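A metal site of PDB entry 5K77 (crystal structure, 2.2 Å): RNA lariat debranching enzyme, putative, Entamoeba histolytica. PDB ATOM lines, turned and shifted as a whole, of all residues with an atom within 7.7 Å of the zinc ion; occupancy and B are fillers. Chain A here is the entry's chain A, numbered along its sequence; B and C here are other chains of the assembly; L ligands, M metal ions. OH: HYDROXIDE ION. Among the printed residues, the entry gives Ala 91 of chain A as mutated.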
ATOM      1  N   GLY A  13      -4.393  -0.651   5.988  1.00  0.00           N
ATOM      2  CA  GLY A  13      -4.712  -1.727   5.066  1.00  0.00           C
ATOM      3  C   GLY A  13      -3.542  -2.635   4.779  1.00  0.00           C
ATOM      4  O   GLY A  13      -2.868  -3.091   5.709  1.00  0.00           O
ATOM      5  N   CYS A  14      -3.268  -2.913   3.500  1.00  0.00           N
ATOM      6  CA  CYS A  14      -2.163  -3.773   3.119  1.00  0.00           C
ATOM      7  C   CYS A  14      -0.852  -3.027   3.217  1.00  0.00           C
ATOM      8  O   CYS A  14      -0.717  -1.913   2.680  1.00  0.00           O
ATOM      9  CB  CYS A  14      -2.370  -4.308   1.699  1.00  0.00           C
ATOM     10  SG  CYS A  14      -3.881  -5.238   1.420  1.00  0.00           S
ATOM     11  N   VAL A  15       0.140  -3.628   3.877  1.00  0.00           N
ATOM     12  CA  VAL A  15       1.468  -3.046   3.963  1.00  0.00           C
ATOM     13  C   VAL A  15       2.350  -3.482   2.800  1.00  0.00           C
ATOM     14  O   VAL A  15       2.995  -2.650   2.161  1.00  0.00           O
ATOM     15  CB  VAL A  15       2.123  -3.391   5.319  1.00  0.00           C
ATOM     16  CG1 VAL A  15       3.597  -3.042   5.306  1.00  0.00           C
ATOM     17  CG2 VAL A  15       1.424  -2.642   6.431  1.00  0.00           C
ATOM     18  N   HIS A  16       2.360  -4.789   2.510  1.00  0.00           N
ATOM     19  CA  HIS A  16       3.151  -5.361   1.422  1.00  0.00           C
ATOM     20  C   HIS A  16       4.623  -4.970   1.538  1.00  0.00           C
ATOM     21  O   HIS A  16       5.283  -4.636   0.555  1.00  0.00           O
ATOM     22  CB  HIS A  16       2.595  -4.965   0.057  1.00  0.00           C
ATOM     23  CG  HIS A  16       1.335  -5.690  -0.315  1.00  0.00           C
ATOM     24  ND1 HIS A  16       1.302  -7.049  -0.551  1.00  0.00           N
ATOM     25  CD2 HIS A  16       0.069  -5.248  -0.487  1.00  0.00           C
ATOM     26  CE1 HIS A  16       0.074  -7.406  -0.851  1.00  0.00           C
ATOM     27  NE2 HIS A  16      -0.699  -6.335  -0.820  1.00  0.00           N
ATOM     28  N   GLY A  44      -3.347  -6.969   7.229  1.00  0.00           N
ATOM     29  CA  GLY A  44      -2.698  -8.137   6.671  1.00  0.00           C
ATOM     30  C   GLY A  44      -1.792  -7.800   5.505  1.00  0.00           C
ATOM     31  O   GLY A  44      -1.547  -6.624   5.186  1.00  0.00           O
ATOM     32  N   ASP A  45      -1.301  -8.850   4.848  1.00  0.00           N
ATOM     33  CA  ASP A  45      -0.285  -8.778   3.801  1.00  0.00           C
ATOM     34  C   ASP A  45       0.943  -8.022   4.298  1.00  0.00           C
ATOM     35  O   ASP A  45       1.387  -7.023   3.723  1.00  0.00           O
ATOM     36  CB  ASP A  45      -0.855  -8.158   2.522  1.00  0.00           C
ATOM     37  CG  ASP A  45      -1.775  -9.106   1.770  1.00  0.00           C
ATOM     38  OD1 ASP A  45      -1.812 -10.306   2.137  1.00  0.00           O
ATOM     39  OD2 ASP A  45      -2.466  -8.676   0.820  1.00  0.00           O
ATOM     40  N   GLN A  47       4.133  -9.434   4.955  1.00  0.00           N
ATOM     41  CA  GLN A  47       5.392  -9.872   4.345  1.00  0.00           C
ATOM     42  C   GLN A  47       6.552  -9.738   5.337  1.00  0.00           C
ATOM     43  O   GLN A  47       7.542  -9.055   5.085  1.00  0.00           O
ATOM     44  CB  GLN A  47       5.672  -9.117   3.043  1.00  0.00           C
ATOM     45  CG  GLN A  47       4.529  -9.166   2.049  1.00  0.00           C
ATOM     46  CD  GLN A  47       4.897  -8.541   0.709  1.00  0.00           C
ATOM     47  OE1 GLN A  47       4.022  -8.298  -0.126  1.00  0.00           O
ATOM     48  NE2 GLN A  47       6.180  -8.287   0.502  1.00  0.00           N
ATOM     49  N   ASN A  90      -2.796 -12.874   2.508  1.00  0.00           N
ATOM     50  CA  ASN A  90      -2.411 -13.881   1.542  1.00  0.00           C
ATOM     51  C   ASN A  90      -0.972 -13.715   1.053  1.00  0.00           C
ATOM     52  O   ASN A  90      -0.437 -14.649   0.438  1.00  0.00           O
ATOM     53  CB  ASN A  90      -3.358 -13.857   0.332  1.00  0.00           C
ATOM     54  CG  ASN A  90      -3.456 -12.485  -0.293  1.00  0.00           C
ATOM     55  OD1 ASN A  90      -4.103 -11.583   0.240  1.00  0.00           O
ATOM     56  ND2 ASN A  90      -2.807 -12.318  -1.439  1.00  0.00           N
ATOM     57  N   ALA A  91      -0.350 -12.578   1.307  1.00  0.00           N
ATOM     58  CA  ALA A  91       1.036 -12.306   0.934  1.00  0.00           C
ATOM     59  C   ALA A  91       1.841 -12.199   2.231  1.00  0.00           C
ATOM     60  O   ALA A  91       1.998 -11.120   2.794  1.00  0.00           O
ATOM     61  CB  ALA A  91       1.150 -11.037   0.089  1.00  0.00           C
ATOM     62  N   HIS A 180      -8.697 -10.041   6.707  1.00  0.00           N
ATOM     63  CA  HIS A 180      -8.006  -9.553   5.523  1.00  0.00           C
ATOM     64  C   HIS A 180      -8.975  -9.326   4.369  1.00  0.00           C
ATOM     65  O   HIS A 180      -9.170  -8.188   3.923  1.00  0.00           O
ATOM     66  CB  HIS A 180      -6.885 -10.517   5.108  1.00  0.00           C
ATOM     67  CG  HIS A 180      -6.013  -9.970   4.031  1.00  0.00           C
ATOM     68  ND1 HIS A 180      -5.264  -8.826   4.191  1.00  0.00           N
ATOM     69  CD2 HIS A 180      -5.785 -10.388   2.754  1.00  0.00           C
ATOM     70  CE1 HIS A 180      -4.610  -8.564   3.077  1.00  0.00           C
ATOM     71  NE2 HIS A 180      -4.897  -9.503   2.193  1.00  0.00           N
ATOM     72  N   GLY A 229      -9.019  -5.445   4.589  1.00  0.00           N
ATOM     73  CA  GLY A 229      -8.202  -4.880   3.545  1.00  0.00           C
ATOM     74  C   GLY A 229      -8.310  -5.649   2.245  1.00  0.00           C
ATOM     75  O   GLY A 229      -9.405  -5.773   1.683  1.00  0.00           O
ATOM     76  N   HIS A 230      -7.179  -6.144   1.755  1.00  0.00           N
ATOM     77  CA  HIS A 230      -7.105  -7.065   0.627  1.00  0.00           C
ATOM     78  C   HIS A 230      -7.490  -6.444  -0.714  1.00  0.00           C
ATOM     79  O   HIS A 230      -6.791  -6.643  -1.704  1.00  0.00           O
ATOM     80  CB  HIS A 230      -7.966  -8.303   0.892  1.00  0.00           C
ATOM     81  CG  HIS A 230      -7.728  -9.426  -0.070  1.00  0.00           C
ATOM     82  ND1 HIS A 230      -6.466  -9.784  -0.504  1.00  0.00           N
ATOM     83  CD2 HIS A 230      -8.592 -10.277  -0.690  1.00  0.00           C
ATOM     84  CE1 HIS A 230      -6.563 -10.801  -1.338  1.00  0.00           C
ATOM     85  NE2 HIS A 230      -7.836 -11.122  -1.470  1.00  0.00           N
ATOM     86  N   MET A 231      -8.587  -5.695  -0.760  1.00  0.00           N
ATOM     87  CA  MET A 231      -9.142  -5.255  -2.036  1.00  0.00           C
ATOM     88  C   MET A 231      -8.521  -3.971  -2.577  1.00  0.00           C
ATOM     89  O   MET A 231      -8.868  -3.555  -3.677  1.00  0.00           O
ATOM     90  CB  MET A 231     -10.663  -5.093  -1.917  1.00  0.00           C
ATOM     91  CG  MET A 231     -11.375  -6.335  -1.390  1.00  0.00           C
ATOM     92  SD  MET A 231     -11.189  -7.795  -2.427  1.00  0.00           S
ATOM     93  CE  MET A 231     -12.340  -7.420  -3.744  1.00  0.00           C
ATOM     94  N   HIS A 232      -7.631  -3.334  -1.816  1.00  0.00           N
ATOM     95  CA  HIS A 232      -6.871  -2.160  -2.289  1.00  0.00           C
ATOM     96  C   HIS A 232      -7.788  -0.993  -2.638  1.00  0.00           C
ATOM     97  O   HIS A 232      -7.600  -0.311  -3.643  1.00  0.00           O
ATOM     98  CB  HIS A 232      -5.989  -2.523  -3.481  1.00  0.00           C
ATOM     99  CG  HIS A 232      -4.925  -3.523  -3.161  1.00  0.00           C
ATOM    100  ND1 HIS A 232      -4.210  -4.177  -4.145  1.00  0.00           N
ATOM    101  CD2 HIS A 232      -4.453  -3.979  -1.981  1.00  0.00           C
ATOM    102  CE1 HIS A 232      -3.334  -4.996  -3.576  1.00  0.00           C
ATOM    103  NE2 HIS A 232      -3.463  -4.897  -2.273  1.00  0.00           N
ATOM    104  N   LEU A 247      -9.816  -0.785   3.718  1.00  0.00           N
ATOM    105  CA  LEU A 247      -8.685   0.105   3.503  1.00  0.00           C
ATOM    106  C   LEU A 247      -7.832  -0.376   2.344  1.00  0.00           C
ATOM    107  O   LEU A 247      -7.747  -1.579   2.073  1.00  0.00           O
ATOM    108  CB  LEU A 247      -7.829   0.223   4.775  1.00  0.00           C
ATOM    109  CG  LEU A 247      -8.570   0.702   6.026  1.00  0.00           C
ATOM    110  CD1 LEU A 247      -7.805   0.320   7.293  1.00  0.00           C
ATOM    111  CD2 LEU A 247      -8.798   2.197   5.961  1.00  0.00           C
ATOM    112  N   GLY A 248      -7.197   0.579   1.650  1.00  0.00           N
ATOM    113  CA  GLY A 248      -6.314   0.282   0.545  1.00  0.00           C
ATOM    114  C   GLY A 248      -4.959  -0.211   1.012  1.00  0.00           C
ATOM    115  O   GLY A 248      -4.801  -0.709   2.135  1.00  0.00           O
ATOM    116  N   LYS A 249      -3.960  -0.063   0.148  1.00  0.00           N
ATOM    117  CA  LYS A 249      -2.613  -0.534   0.453  1.00  0.00           C
ATOM    118  C   LYS A 249      -1.649   0.642   0.555  1.00  0.00           C
ATOM    119  O   LYS A 249      -1.812   1.664  -0.108  1.00  0.00           O
ATOM    120  CB  LYS A 249      -2.112  -1.553  -0.583  1.00  0.00           C
ATOM    121  CG  LYS A 249      -1.926  -1.033  -1.992  1.00  0.00           C
ATOM    122  CD  LYS A 249      -1.208  -2.094  -2.827  1.00  0.00           C
ATOM    123  CE  LYS A 249      -1.239  -1.785  -4.310  1.00  0.00           C
ATOM    124  NZ  LYS A 249      -0.527  -2.834  -5.088  1.00  0.00           N
ATOM    125  N   ILE A 250      -0.627   0.455   1.408  1.00  0.00           N
ATOM    126  CA  ILE A 250       0.371   1.497   1.636  1.00  0.00           C
ATOM    127  C   ILE A 250       1.006   1.909   0.318  1.00  0.00           C
ATOM    128  O   ILE A 250       1.238   1.080  -0.578  1.00  0.00           O
ATOM    129  CB  ILE A 250       1.432   0.998   2.642  1.00  0.00           C
ATOM    130  CG1 ILE A 250       0.781   0.711   3.991  1.00  0.00           C
ATOM    131  CG2 ILE A 250       2.547   2.015   2.806  1.00  0.00           C
ATOM    132  CD1 ILE A 250       0.220   1.939   4.670  1.00  0.00           C
ATOM    133  OP3   G B   1      -2.322  -9.907  -4.265  1.00  0.00           O
ATOM    134  P     G B   1      -3.380  -9.275  -3.249  1.00  0.00           P
ATOM    135  OP1   G B   1      -3.032  -7.839  -3.092  1.00  0.00           O
ATOM    136  OP2   G B   1      -3.449 -10.114  -2.034  1.00  0.00           O
ATOM    137  O5'   G B   1      -4.805  -9.358  -3.967  1.00  0.00           O
ATOM    138  C5'   G B   1      -5.640  -8.214  -4.075  1.00  0.00           C
ATOM    139  C4'   G B   1      -6.205  -8.052  -5.466  1.00  0.00           C
ATOM    140  O4'   G B   1      -7.149  -9.130  -5.734  1.00  0.00           O
ATOM    141  C3'   G B   1      -6.976  -6.748  -5.695  1.00  0.00           C
ATOM    142  O3'   G B   1      -6.810  -6.342  -7.048  1.00  0.00           O
ATOM    143  C2'   G B   1      -8.415  -7.168  -5.459  1.00  0.00           C
ATOM    144  O2'   G B   1      -9.377  -6.345  -6.085  1.00  0.00           O
ATOM    145  C1'   G B   1      -8.418  -8.577  -6.048  1.00  0.00           C
ATOM    146  N9    G B   1      -9.455  -9.464  -5.508  1.00  0.00           N
ATOM    147  C8    G B   1      -9.388 -10.245  -4.381  1.00  0.00           C
ATOM    148  N7    G B   1     -10.475 -10.944  -4.162  1.00  0.00           N
ATOM    149  C5    G B   1     -11.316 -10.595  -5.213  1.00  0.00           C
ATOM    150  C6    G B   1     -12.631 -11.019  -5.520  1.00  0.00           C
ATOM    151  O6    G B   1     -13.346 -11.818  -4.897  1.00  0.00           O
ATOM    152  N1    G B   1     -13.111 -10.423  -6.675  1.00  0.00           N
ATOM    153  C2    G B   1     -12.418  -9.524  -7.446  1.00  0.00           C
ATOM    154  N2    G B   1     -13.049  -9.054  -8.537  1.00  0.00           N
ATOM    155  N3    G B   1     -11.189  -9.113  -7.181  1.00  0.00           N
ATOM    156  C4    G B   1     -10.698  -9.689  -6.050  1.00  0.00           C
ATOM    157  P     U B   2      -5.616  -5.358  -7.470  1.00  0.00           P
ATOM    158  OP1   U B   2      -4.343  -6.002  -7.038  1.00  0.00           O
ATOM    159  OP2   U B   2      -5.960  -4.028  -6.900  1.00  0.00           O
ATOM    160  O5'   U B   2      -5.690  -5.325  -9.050  1.00  0.00           O
ATOM    161  P     A C   3      -1.203  -8.420 -11.035  1.00  0.00           P
ATOM    162  OP1   A C   3      -1.317  -7.163 -11.795  1.00  0.00           O
ATOM    163  OP2   A C   3       0.020  -9.245 -11.153  1.00  0.00           O
ATOM    164  O5'   A C   3      -1.421  -8.093  -9.482  1.00  0.00           O
ATOM    165  C5'   A C   3      -2.410  -8.804  -8.731  1.00  0.00           C
ATOM    166  C4'   A C   3      -1.761  -9.865  -7.858  1.00  0.00           C
ATOM    167  O4'   A C   3      -0.543  -9.331  -7.267  1.00  0.00           O
ATOM    168  C3'   A C   3      -2.612 -10.336  -6.691  1.00  0.00           C
ATOM    169  O3'   A C   3      -2.318 -11.695  -6.386  1.00  0.00           O
ATOM    170  C2'   A C   3      -2.154  -9.404  -5.564  1.00  0.00           C
ATOM    171  C1'   A C   3      -0.669  -9.276  -5.863  1.00  0.00           C
ATOM    172  N9    A C   3      -0.079  -8.027  -5.382  1.00  0.00           N
ATOM    173  C8    A C   3      -0.468  -6.756  -5.723  1.00  0.00           C
ATOM    174  N7    A C   3       0.256  -5.825  -5.149  1.00  0.00           N
ATOM    175  C5    A C   3       1.173  -6.525  -4.390  1.00  0.00           C
ATOM    176  C6    A C   3       2.225  -6.114  -3.556  1.00  0.00           C
ATOM    177  N6    A C   3       2.533  -4.830  -3.326  1.00  0.00           N
ATOM    178  N1    A C   3       2.963  -7.071  -2.948  1.00  0.00           N
ATOM    179  C2    A C   3       2.655  -8.357  -3.168  1.00  0.00           C
ATOM    180  N3    A C   3       1.691  -8.867  -3.945  1.00  0.00           N
ATOM    181  C4    A C   3       0.981  -7.884  -4.531  1.00  0.00           C
HETATM  182  O    OH L   1      -4.369  -7.683  -0.786  1.00  0.00           O
HETATM  183 ZN    ZN M   1      -2.937  -6.297  -0.719  1.00  0.00          ZN
HETATM  184 FE    FE M   2      -4.270  -9.494   0.020  1.00  0.00          FE
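Merely in contact with the zinc ion: Asp 45 (2.9 Å) and His 230 (3.99 Å).
Six residues have an atom within 4 Å of the zinc ion: Cys 14, His 16, Asp 45, His 230, His 232 and G 1 of chain B.
O of the ligand is bound to the zinc ion.
NE2 of His 232 binds the zinc ion, at 2.2 Å.
The zinc ion is bound by NE2 of His 16 (2.2 Å).
The zinc ion is bound by SG of Cys 14 (2.6 Å).
The zinc ion has four donor atoms within binding distance.
Slightly farther from the zinc ion lies OP1 of G 1 of chain B (2.8 Å).
A ring nitrogen (ND1) of His 232 is in hydrogen-bond range of OP2 of U 2 of chain B.
A ring nitrogen (ND1) of His 16 lies within hydrogen-bond range of the side-chain amide oxygen of Gln 47 (3.0 Å).
The side-chain sulfur (SG) of Cys 14 lies close to the backbone NH (N) of His 230 (3.4 Å).
OP1 of G 1 of chain B lies close to NE2 of His 232, 3.1 Å away.
The side-chain carboxylate of Asp 45 lies within hydrogen-bond range of the backbone NH of Ala 91, at 2.8 Å.
OP3 of G 1 of chain B is covalently linked to C2' of A 3 of chain C (1.4 Å).
O of Gly 248 is in hydrogen-bond range of N of Cys 14.
The backbone NH (N) of Ile 250 lies within hydrogen-bond range of the backbone carbonyl oxygen (O) of Cys 14, at 2.7 Å.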
